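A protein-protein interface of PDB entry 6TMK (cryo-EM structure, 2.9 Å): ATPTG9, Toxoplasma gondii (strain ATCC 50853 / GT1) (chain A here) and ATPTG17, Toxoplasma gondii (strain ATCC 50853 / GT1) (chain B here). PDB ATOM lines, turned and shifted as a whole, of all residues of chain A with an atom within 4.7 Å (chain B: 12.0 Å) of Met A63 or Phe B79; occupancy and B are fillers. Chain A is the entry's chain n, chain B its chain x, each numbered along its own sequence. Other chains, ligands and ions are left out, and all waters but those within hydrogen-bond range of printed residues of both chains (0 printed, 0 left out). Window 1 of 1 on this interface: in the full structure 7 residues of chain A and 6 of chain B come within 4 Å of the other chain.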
ATOM      1  N   LEU A  25      -2.954  19.455 -25.247  1.00  0.00           N
ATOM      2  CA  LEU A  25      -4.078  19.459 -24.322  1.00  0.00           C
ATOM      3  C   LEU A  25      -4.840  20.775 -24.393  1.00  0.00           C
ATOM      4  O   LEU A  25      -6.074  20.787 -24.372  1.00  0.00           O
ATOM      5  CB  LEU A  25      -3.567  19.209 -22.906  1.00  0.00           C
ATOM      6  CG  LEU A  25      -4.481  18.547 -21.881  1.00  0.00           C
ATOM      7  CD1 LEU A  25      -5.147  17.312 -22.437  1.00  0.00           C
ATOM      8  CD2 LEU A  25      -3.667  18.192 -20.665  1.00  0.00           C
ATOM      9  N   ARG A  30     -10.482  20.827 -22.292  1.00  0.00           N
ATOM     10  CA  ARG A  30     -10.687  19.967 -21.135  1.00  0.00           C
ATOM     11  C   ARG A  30     -11.938  19.108 -21.249  1.00  0.00           C
ATOM     12  O   ARG A  30     -12.188  18.285 -20.364  1.00  0.00           O
ATOM     13  CB  ARG A  30     -10.743  20.797 -19.851  1.00  0.00           C
ATOM     14  CG  ARG A  30     -11.869  21.793 -19.750  1.00  0.00           C
ATOM     15  CD  ARG A  30     -12.178  22.043 -18.293  1.00  0.00           C
ATOM     16  NE  ARG A  30     -13.063  23.179 -18.065  1.00  0.00           N
ATOM     17  CZ  ARG A  30     -12.662  24.444 -18.035  1.00  0.00           C
ATOM     18  NH1 ARG A  30     -11.394  24.749 -18.230  1.00  0.00           N
ATOM     19  NH2 ARG A  30     -13.532  25.409 -17.815  1.00  0.00           N
ATOM     20  N   PHE A  33     -10.178  15.389 -23.567  1.00  0.00           N
ATOM     21  CA  PHE A  33      -8.865  15.151 -22.989  1.00  0.00           C
ATOM     22  C   PHE A  33      -8.380  13.720 -23.155  1.00  0.00           C
ATOM     23  O   PHE A  33      -7.196  13.456 -22.918  1.00  0.00           O
ATOM     24  CB  PHE A  33      -8.874  15.500 -21.494  1.00  0.00           C
ATOM     25  CG  PHE A  33      -9.919  14.771 -20.711  1.00  0.00           C
ATOM     26  CD1 PHE A  33      -9.656  13.524 -20.176  1.00  0.00           C
ATOM     27  CD2 PHE A  33     -11.165  15.329 -20.508  1.00  0.00           C
ATOM     28  CE1 PHE A  33     -10.615  12.850 -19.458  1.00  0.00           C
ATOM     29  CE2 PHE A  33     -12.128  14.659 -19.789  1.00  0.00           C
ATOM     30  CZ  PHE A  33     -11.852  13.417 -19.263  1.00  0.00           C
ATOM     31  N   GLY A  59      -4.340  15.918 -13.037  1.00  0.00           N
ATOM     32  CA  GLY A  59      -5.008  16.662 -14.088  1.00  0.00           C
ATOM     33  C   GLY A  59      -6.132  15.874 -14.729  1.00  0.00           C
ATOM     34  O   GLY A  59      -7.223  16.402 -14.966  1.00  0.00           O
ATOM     35  N   ILE A  60      -5.883  14.596 -15.012  1.00  0.00           N
ATOM     36  CA  ILE A  60      -6.898  13.772 -15.657  1.00  0.00           C
ATOM     37  C   ILE A  60      -8.101  13.589 -14.741  1.00  0.00           C
ATOM     38  O   ILE A  60      -9.253  13.672 -15.184  1.00  0.00           O
ATOM     39  CB  ILE A  60      -6.289  12.423 -16.072  1.00  0.00           C
ATOM     40  CG1 ILE A  60      -5.276  12.624 -17.199  1.00  0.00           C
ATOM     41  CG2 ILE A  60      -7.369  11.467 -16.505  1.00  0.00           C
ATOM     42  CD1 ILE A  60      -5.866  13.185 -18.474  1.00  0.00           C
ATOM     43  N   ASN A  61      -7.858  13.336 -13.456  1.00  0.00           N
ATOM     44  CA  ASN A  61      -8.961  13.155 -12.523  1.00  0.00           C
ATOM     45  C   ASN A  61      -9.780  14.429 -12.403  1.00  0.00           C
ATOM     46  O   ASN A  61     -11.013  14.381 -12.351  1.00  0.00           O
ATOM     47  CB  ASN A  61      -8.428  12.729 -11.159  1.00  0.00           C
ATOM     48  CG  ASN A  61      -7.917  11.311 -11.155  1.00  0.00           C
ATOM     49  OD1 ASN A  61      -8.403  10.459 -11.898  1.00  0.00           O
ATOM     50  ND2 ASN A  61      -6.930  11.044 -10.312  1.00  0.00           N
ATOM     51  N   LEU A  62      -9.113  15.583 -12.358  1.00  0.00           N
ATOM     52  CA  LEU A  62      -9.832  16.848 -12.284  1.00  0.00           C
ATOM     53  C   LEU A  62     -10.698  17.060 -13.517  1.00  0.00           C
ATOM     54  O   LEU A  62     -11.871  17.446 -13.415  1.00  0.00           O
ATOM     55  CB  LEU A  62      -8.838  17.993 -12.131  1.00  0.00           C
ATOM     56  CG  LEU A  62      -9.438  19.389 -12.013  1.00  0.00           C
ATOM     57  CD1 LEU A  62     -10.258  19.507 -10.764  1.00  0.00           C
ATOM     58  CD2 LEU A  62      -8.348  20.414 -12.026  1.00  0.00           C
ATOM     59  N   MET A  63     -10.124  16.834 -14.698  1.00  0.00           N
ATOM     60  CA  MET A  63     -10.881  17.008 -15.930  1.00  0.00           C
ATOM     61  C   MET A  63     -12.087  16.083 -15.969  1.00  0.00           C
ATOM     62  O   MET A  63     -13.180  16.492 -16.377  1.00  0.00           O
ATOM     63  CB  MET A  63      -9.977  16.748 -17.127  1.00  0.00           C
ATOM     64  CG  MET A  63      -9.010  17.863 -17.426  1.00  0.00           C
ATOM     65  SD  MET A  63      -7.626  17.278 -18.412  1.00  0.00           S
ATOM     66  CE  MET A  63      -7.249  18.753 -19.336  1.00  0.00           C
ATOM     67  N   LYS A  64     -11.910  14.828 -15.554  1.00  0.00           N
ATOM     68  CA  LYS A  64     -13.027  13.893 -15.545  1.00  0.00           C
ATOM     69  C   LYS A  64     -14.097  14.317 -14.548  1.00  0.00           C
ATOM     70  O   LYS A  64     -15.295  14.226 -14.838  1.00  0.00           O
ATOM     71  CB  LYS A  64     -12.529  12.488 -15.217  1.00  0.00           C
ATOM     72  CG  LYS A  64     -11.825  11.797 -16.365  1.00  0.00           C
ATOM     73  CD  LYS A  64     -11.121  10.535 -15.909  1.00  0.00           C
ATOM     74  CE  LYS A  64     -10.415   9.851 -17.067  1.00  0.00           C
ATOM     75  NZ  LYS A  64      -9.467   8.797 -16.614  1.00  0.00           N
ATOM     76  N   CYS A  65     -13.684  14.786 -13.371  1.00  0.00           N
ATOM     77  CA  CYS A  65     -14.647  15.116 -12.327  1.00  0.00           C
ATOM     78  C   CYS A  65     -15.465  16.349 -12.684  1.00  0.00           C
ATOM     79  O   CYS A  65     -16.677  16.381 -12.447  1.00  0.00           O
ATOM     80  CB  CYS A  65     -13.922  15.320 -11.000  1.00  0.00           C
ATOM     81  SG  CYS A  65     -13.400  13.785 -10.202  1.00  0.00           S
ATOM     82  N   THR A  66     -14.831  17.376 -13.252  1.00  0.00           N
ATOM     83  CA  THR A  66     -15.532  18.643 -13.429  1.00  0.00           C
ATOM     84  C   THR A  66     -16.676  18.555 -14.428  1.00  0.00           C
ATOM     85  O   THR A  66     -17.527  19.450 -14.449  1.00  0.00           O
ATOM     86  CB  THR A  66     -14.567  19.739 -13.860  1.00  0.00           C
ATOM     87  OG1 THR A  66     -13.815  19.311 -14.998  1.00  0.00           O
ATOM     88  CG2 THR A  66     -13.636  20.069 -12.725  1.00  0.00           C
ATOM     89  N   LYS A  67     -16.719  17.515 -15.256  1.00  0.00           N
ATOM     90  CA  LYS A  67     -17.835  17.339 -16.173  1.00  0.00           C
ATOM     91  C   LYS A  67     -18.954  16.498 -15.577  1.00  0.00           C
ATOM     92  O   LYS A  67     -20.103  16.621 -16.014  1.00  0.00           O
ATOM     93  CB  LYS A  67     -17.358  16.705 -17.481  1.00  0.00           C
ATOM     94  CG  LYS A  67     -16.599  15.407 -17.316  1.00  0.00           C
ATOM     95  CD  LYS A  67     -16.703  14.561 -18.566  1.00  0.00           C
ATOM     96  CE  LYS A  67     -16.087  15.265 -19.760  1.00  0.00           C
ATOM     97  NZ  LYS A  67     -16.053  14.393 -20.959  1.00  0.00           N
ATOM     98  N   MET A  81      -4.331  19.004  -7.347  1.00  0.00           N
ATOM     99  CA  MET A  81      -3.606  19.497  -8.510  1.00  0.00           C
ATOM    100  C   MET A  81      -2.735  20.690  -8.144  1.00  0.00           C
ATOM    101  O   MET A  81      -1.568  20.777  -8.558  1.00  0.00           O
ATOM    102  CB  MET A  81      -4.591  19.867  -9.615  1.00  0.00           C
ATOM    103  CG  MET A  81      -3.944  20.246 -10.925  1.00  0.00           C
ATOM    104  SD  MET A  81      -2.981  18.912 -11.650  1.00  0.00           S
ATOM    105  CE  MET A  81      -1.915  19.846 -12.738  1.00  0.00           C
ATOM    106  N   SER B  47     -18.915  30.676 -24.205  1.00  0.00           N
ATOM    107  CA  SER B  47     -17.585  30.467 -23.647  1.00  0.00           C
ATOM    108  C   SER B  47     -17.607  30.662 -22.138  1.00  0.00           C
ATOM    109  O   SER B  47     -17.288  29.745 -21.374  1.00  0.00           O
ATOM    110  CB  SER B  47     -16.586  31.416 -24.308  1.00  0.00           C
ATOM    111  OG  SER B  47     -15.259  31.087 -23.946  1.00  0.00           O
ATOM    112  N   TYR B  72      -4.152  37.992 -17.464  1.00  0.00           N
ATOM    113  CA  TYR B  72      -3.464  36.729 -17.719  1.00  0.00           C
ATOM    114  C   TYR B  72      -4.165  35.921 -18.806  1.00  0.00           C
ATOM    115  O   TYR B  72      -4.337  34.707 -18.690  1.00  0.00           O
ATOM    116  CB  TYR B  72      -3.349  35.914 -16.432  1.00  0.00           C
ATOM    117  CG  TYR B  72      -2.937  36.733 -15.240  1.00  0.00           C
ATOM    118  CD1 TYR B  72      -1.862  37.597 -15.308  1.00  0.00           C
ATOM    119  CD2 TYR B  72      -3.626  36.644 -14.046  1.00  0.00           C
ATOM    120  CE1 TYR B  72      -1.487  38.350 -14.222  1.00  0.00           C
ATOM    121  CE2 TYR B  72      -3.258  37.391 -12.958  1.00  0.00           C
ATOM    122  CZ  TYR B  72      -2.186  38.241 -13.050  1.00  0.00           C
ATOM    123  OH  TYR B  72      -1.806  38.998 -11.968  1.00  0.00           O
ATOM    124  N   ASN B  73      -4.571  36.603 -19.875  1.00  0.00           N
ATOM    125  CA  ASN B  73      -5.316  35.989 -20.966  1.00  0.00           C
ATOM    126  C   ASN B  73      -4.559  36.026 -22.287  1.00  0.00           C
ATOM    127  O   ASN B  73      -5.153  35.759 -23.336  1.00  0.00           O
ATOM    128  CB  ASN B  73      -6.673  36.674 -21.124  1.00  0.00           C
ATOM    129  CG  ASN B  73      -7.724  35.756 -21.696  1.00  0.00           C
ATOM    130  OD1 ASN B  73      -7.858  34.609 -21.275  1.00  0.00           O
ATOM    131  ND2 ASN B  73      -8.478  36.257 -22.661  1.00  0.00           N
ATOM    132  N   GLY B  75      -1.739  34.163 -23.143  1.00  0.00           N
ATOM    133  CA  GLY B  75      -1.304  32.842 -23.532  1.00  0.00           C
ATOM    134  C   GLY B  75      -2.434  31.828 -23.491  1.00  0.00           C
ATOM    135  O   GLY B  75      -3.603  32.153 -23.277  1.00  0.00           O
ATOM    136  N   GLU B  76      -2.062  30.571 -23.707  1.00  0.00           N
ATOM    137  CA  GLU B  76      -2.995  29.458 -23.672  1.00  0.00           C
ATOM    138  C   GLU B  76      -2.676  28.539 -22.502  1.00  0.00           C
ATOM    139  O   GLU B  76      -1.534  28.469 -22.038  1.00  0.00           O
ATOM    140  CB  GLU B  76      -2.949  28.668 -24.977  1.00  0.00           C
ATOM    141  CG  GLU B  76      -4.229  27.935 -25.286  1.00  0.00           C
ATOM    142  CD  GLU B  76      -5.358  28.875 -25.661  1.00  0.00           C
ATOM    143  OE1 GLU B  76      -6.511  28.409 -25.773  1.00  0.00           O
ATOM    144  OE2 GLU B  76      -5.090  30.080 -25.839  1.00  0.00           O
ATOM    145  N   TRP B  77      -3.700  27.835 -22.028  1.00  0.00           N
ATOM    146  CA  TRP B  77      -3.619  27.074 -20.793  1.00  0.00           C
ATOM    147  C   TRP B  77      -4.042  25.634 -21.039  1.00  0.00           C
ATOM    148  O   TRP B  77      -4.959  25.370 -21.820  1.00  0.00           O
ATOM    149  CB  TRP B  77      -4.496  27.715 -19.722  1.00  0.00           C
ATOM    150  CG  TRP B  77      -4.320  27.152 -18.364  1.00  0.00           C
ATOM    151  CD1 TRP B  77      -3.165  26.722 -17.798  1.00  0.00           C
ATOM    152  CD2 TRP B  77      -5.339  26.972 -17.383  1.00  0.00           C
ATOM    153  NE1 TRP B  77      -3.400  26.277 -16.524  1.00  0.00           N
ATOM    154  CE2 TRP B  77      -4.732  26.421 -16.247  1.00  0.00           C
ATOM    155  CE3 TRP B  77      -6.709  27.222 -17.356  1.00  0.00           C
ATOM    156  CZ2 TRP B  77      -5.444  26.116 -15.101  1.00  0.00           C
ATOM    157  CZ3 TRP B  77      -7.410  26.917 -16.223  1.00  0.00           C
ATOM    158  CH2 TRP B  77      -6.782  26.372 -15.110  1.00  0.00           C
ATOM    159  N   MET B  78      -3.367  24.709 -20.355  1.00  0.00           N
ATOM    160  CA  MET B  78      -3.581  23.289 -20.608  1.00  0.00           C
ATOM    161  C   MET B  78      -5.002  22.862 -20.262  1.00  0.00           C
ATOM    162  O   MET B  78      -5.596  22.033 -20.961  1.00  0.00           O
ATOM    163  CB  MET B  78      -2.564  22.463 -19.824  1.00  0.00           C
ATOM    164  CG  MET B  78      -2.555  22.715 -18.338  1.00  0.00           C
ATOM    165  SD  MET B  78      -1.252  21.804 -17.496  1.00  0.00           S
ATOM    166  CE  MET B  78      -1.933  20.153 -17.536  1.00  0.00           C
ATOM    167  N   PHE B  79      -5.564  23.409 -19.191  1.00  0.00           N
ATOM    168  CA  PHE B  79      -6.929  23.092 -18.794  1.00  0.00           C
ATOM    169  C   PHE B  79      -7.970  23.888 -19.564  1.00  0.00           C
ATOM    170  O   PHE B  79      -9.154  23.825 -19.224  1.00  0.00           O
ATOM    171  CB  PHE B  79      -7.109  23.333 -17.296  1.00  0.00           C
ATOM    172  CG  PHE B  79      -6.389  22.344 -16.436  1.00  0.00           C
ATOM    173  CD1 PHE B  79      -6.874  21.063 -16.279  1.00  0.00           C
ATOM    174  CD2 PHE B  79      -5.225  22.694 -15.787  1.00  0.00           C
ATOM    175  CE1 PHE B  79      -6.211  20.155 -15.492  1.00  0.00           C
ATOM    176  CE2 PHE B  79      -4.561  21.791 -15.001  1.00  0.00           C
ATOM    177  CZ  PHE B  79      -5.053  20.519 -14.853  1.00  0.00           C
ATOM    178  N   GLY B  80      -7.558  24.638 -20.573  1.00  0.00           N
ATOM    179  CA  GLY B  80      -8.492  25.293 -21.472  1.00  0.00           C
ATOM    180  C   GLY B  80      -8.747  26.735 -21.065  1.00  0.00           C
ATOM    181  O   GLY B  80      -7.813  27.486 -20.791  1.00  0.00           O
ATOM    182  N   ASN B  81     -10.018  27.120 -21.037  1.00  0.00           N
ATOM    183  CA  ASN B  81     -10.375  28.464 -20.614  1.00  0.00           C
ATOM    184  C   ASN B  81      -9.983  28.685 -19.161  1.00  0.00           C
ATOM    185  O   ASN B  81      -9.981  27.763 -18.344  1.00  0.00           O
ATOM    186  CB  ASN B  81     -11.869  28.701 -20.794  1.00  0.00           C
ATOM    187  CG  ASN B  81     -12.252  28.907 -22.237  1.00  0.00           C
ATOM    188  OD1 ASN B  81     -11.476  29.446 -23.026  1.00  0.00           O
ATOM    189  ND2 ASN B  81     -13.458  28.486 -22.595  1.00  0.00           N
ATOM    190  N   SER B  82      -9.664  29.932 -18.843  1.00  0.00           N
ATOM    191  CA  SER B  82      -9.263  30.310 -17.500  1.00  0.00           C
ATOM    192  C   SER B  82     -10.446  30.591 -16.596  1.00  0.00           C
ATOM    193  O   SER B  82     -10.295  31.284 -15.585  1.00  0.00           O
ATOM    194  CB  SER B  82      -8.363  31.537 -17.574  1.00  0.00           C
ATOM    195  OG  SER B  82      -7.352  31.357 -18.546  1.00  0.00           O
ATOM    196  N   TYR B  83     -11.616  30.068 -16.939  1.00  0.00           N
ATOM    197  CA  TYR B  83     -12.846  30.409 -16.246  1.00  0.00           C
ATOM    198  C   TYR B  83     -13.904  29.332 -16.443  1.00  0.00           C
ATOM    199  O   TYR B  83     -13.634  28.286 -17.028  1.00  0.00           O
ATOM    200  CB  TYR B  83     -13.363  31.769 -16.718  1.00  0.00           C
ATOM    201  CG  TYR B  83     -13.321  31.984 -18.209  1.00  0.00           C
ATOM    202  CD1 TYR B  83     -12.321  32.744 -18.784  1.00  0.00           C
ATOM    203  CD2 TYR B  83     -14.284  31.445 -19.036  1.00  0.00           C
ATOM    204  CE1 TYR B  83     -12.275  32.949 -20.138  1.00  0.00           C
ATOM    205  CE2 TYR B  83     -14.245  31.647 -20.393  1.00  0.00           C
ATOM    206  CZ  TYR B  83     -13.239  32.400 -20.940  1.00  0.00           C
ATOM    207  OH  TYR B  83     -13.197  32.606 -22.297  1.00  0.00           O
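The guanidinium group (NH1) of Arg A30 lies within hydrogen-bond range of the backbone carbonyl oxygen (O) of Phe B79 (2.6 Å).
NH1 of Arg A30 lies within hydrogen-bond range of O of Asn B81 (3.3 Å).
The guanidinium group of Arg A30 is in hydrogen-bond range of the backbone carbonyl oxygen of Tyr B83, at 3.0 Å.
The side-chain hydroxyl of Ser B47 lies within hydrogen-bond range of the side-chain amide nitrogen of Asn B81.
The side-chain hydroxyl (OH) of Tyr B83 is in hydrogen-bond range of the side-chain hydroxyl (OG) of Ser B47 (3.0 Å).
The side-chain sulfur (SD) of Met A81 lies within hydrogen-bond range of the backbone NH (N) of Gly A59 (3.6 Å).
OG1 of Thr A66 is in hydrogen-bond range of O of Met A63 (3.2 Å).
Leu A25 touches Met B78.
CE1 of Phe B79 touches O of Gly A59, at 3.9 Å.
CE of Met A63 touches CD1 of Phe B79, 3.8 Å away.
Met A81 touches Phe B79 (CE to CZ, 3.8 Å).
Arg A30 touches three residues of chain B.
Phe A33 touches none of the printed residues of chain B.
Gly A59 touches just one residue of chain B: Phe B79 (3.9 Å).
No residue of chain B comes within 4 Å of Ile A60.
No residue of chain B comes within 4 Å of Asn A61.
Leu A62 touches none of the printed residues of chain B.
Of the printed residues of chain B, Met A63 touches Phe B79 (3.8 Å).
No residue of chain B comes within 4 Å of Cys A65.
No residue of chain B comes within 4 Å of Thr A66.
No residue of chain B comes within 4 Å of Lys A67.
Ser B47 touches none of the printed residues of chain A.
Asn B73 touches none of the printed residues of chain A.
Phe B79 touches four residues of chain A.
Printed residues of chain A within 4 Å of Asn B81: Arg A30.
Of the printed residues of chain A, Tyr B83 touches Arg A30.
Of the 12 printed residues of chain B, 4 touch a printed residue of chain A.
Printed residues of chain B that touch a printed residue of chain A: Met B78, Phe B79, Asn B81 and Tyr B83.
Hydrophobic or aromatic side chains of chain B within 4 Å of the printed part of chain A: Phe B79.
Of the 13 printed residues of chain A, 5 touch a printed residue of chain B.
Among the printed residues, no Asp or Glu carboxylate lies within 4 Å of a Lys or Arg side-chain nitrogen of the other chain.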
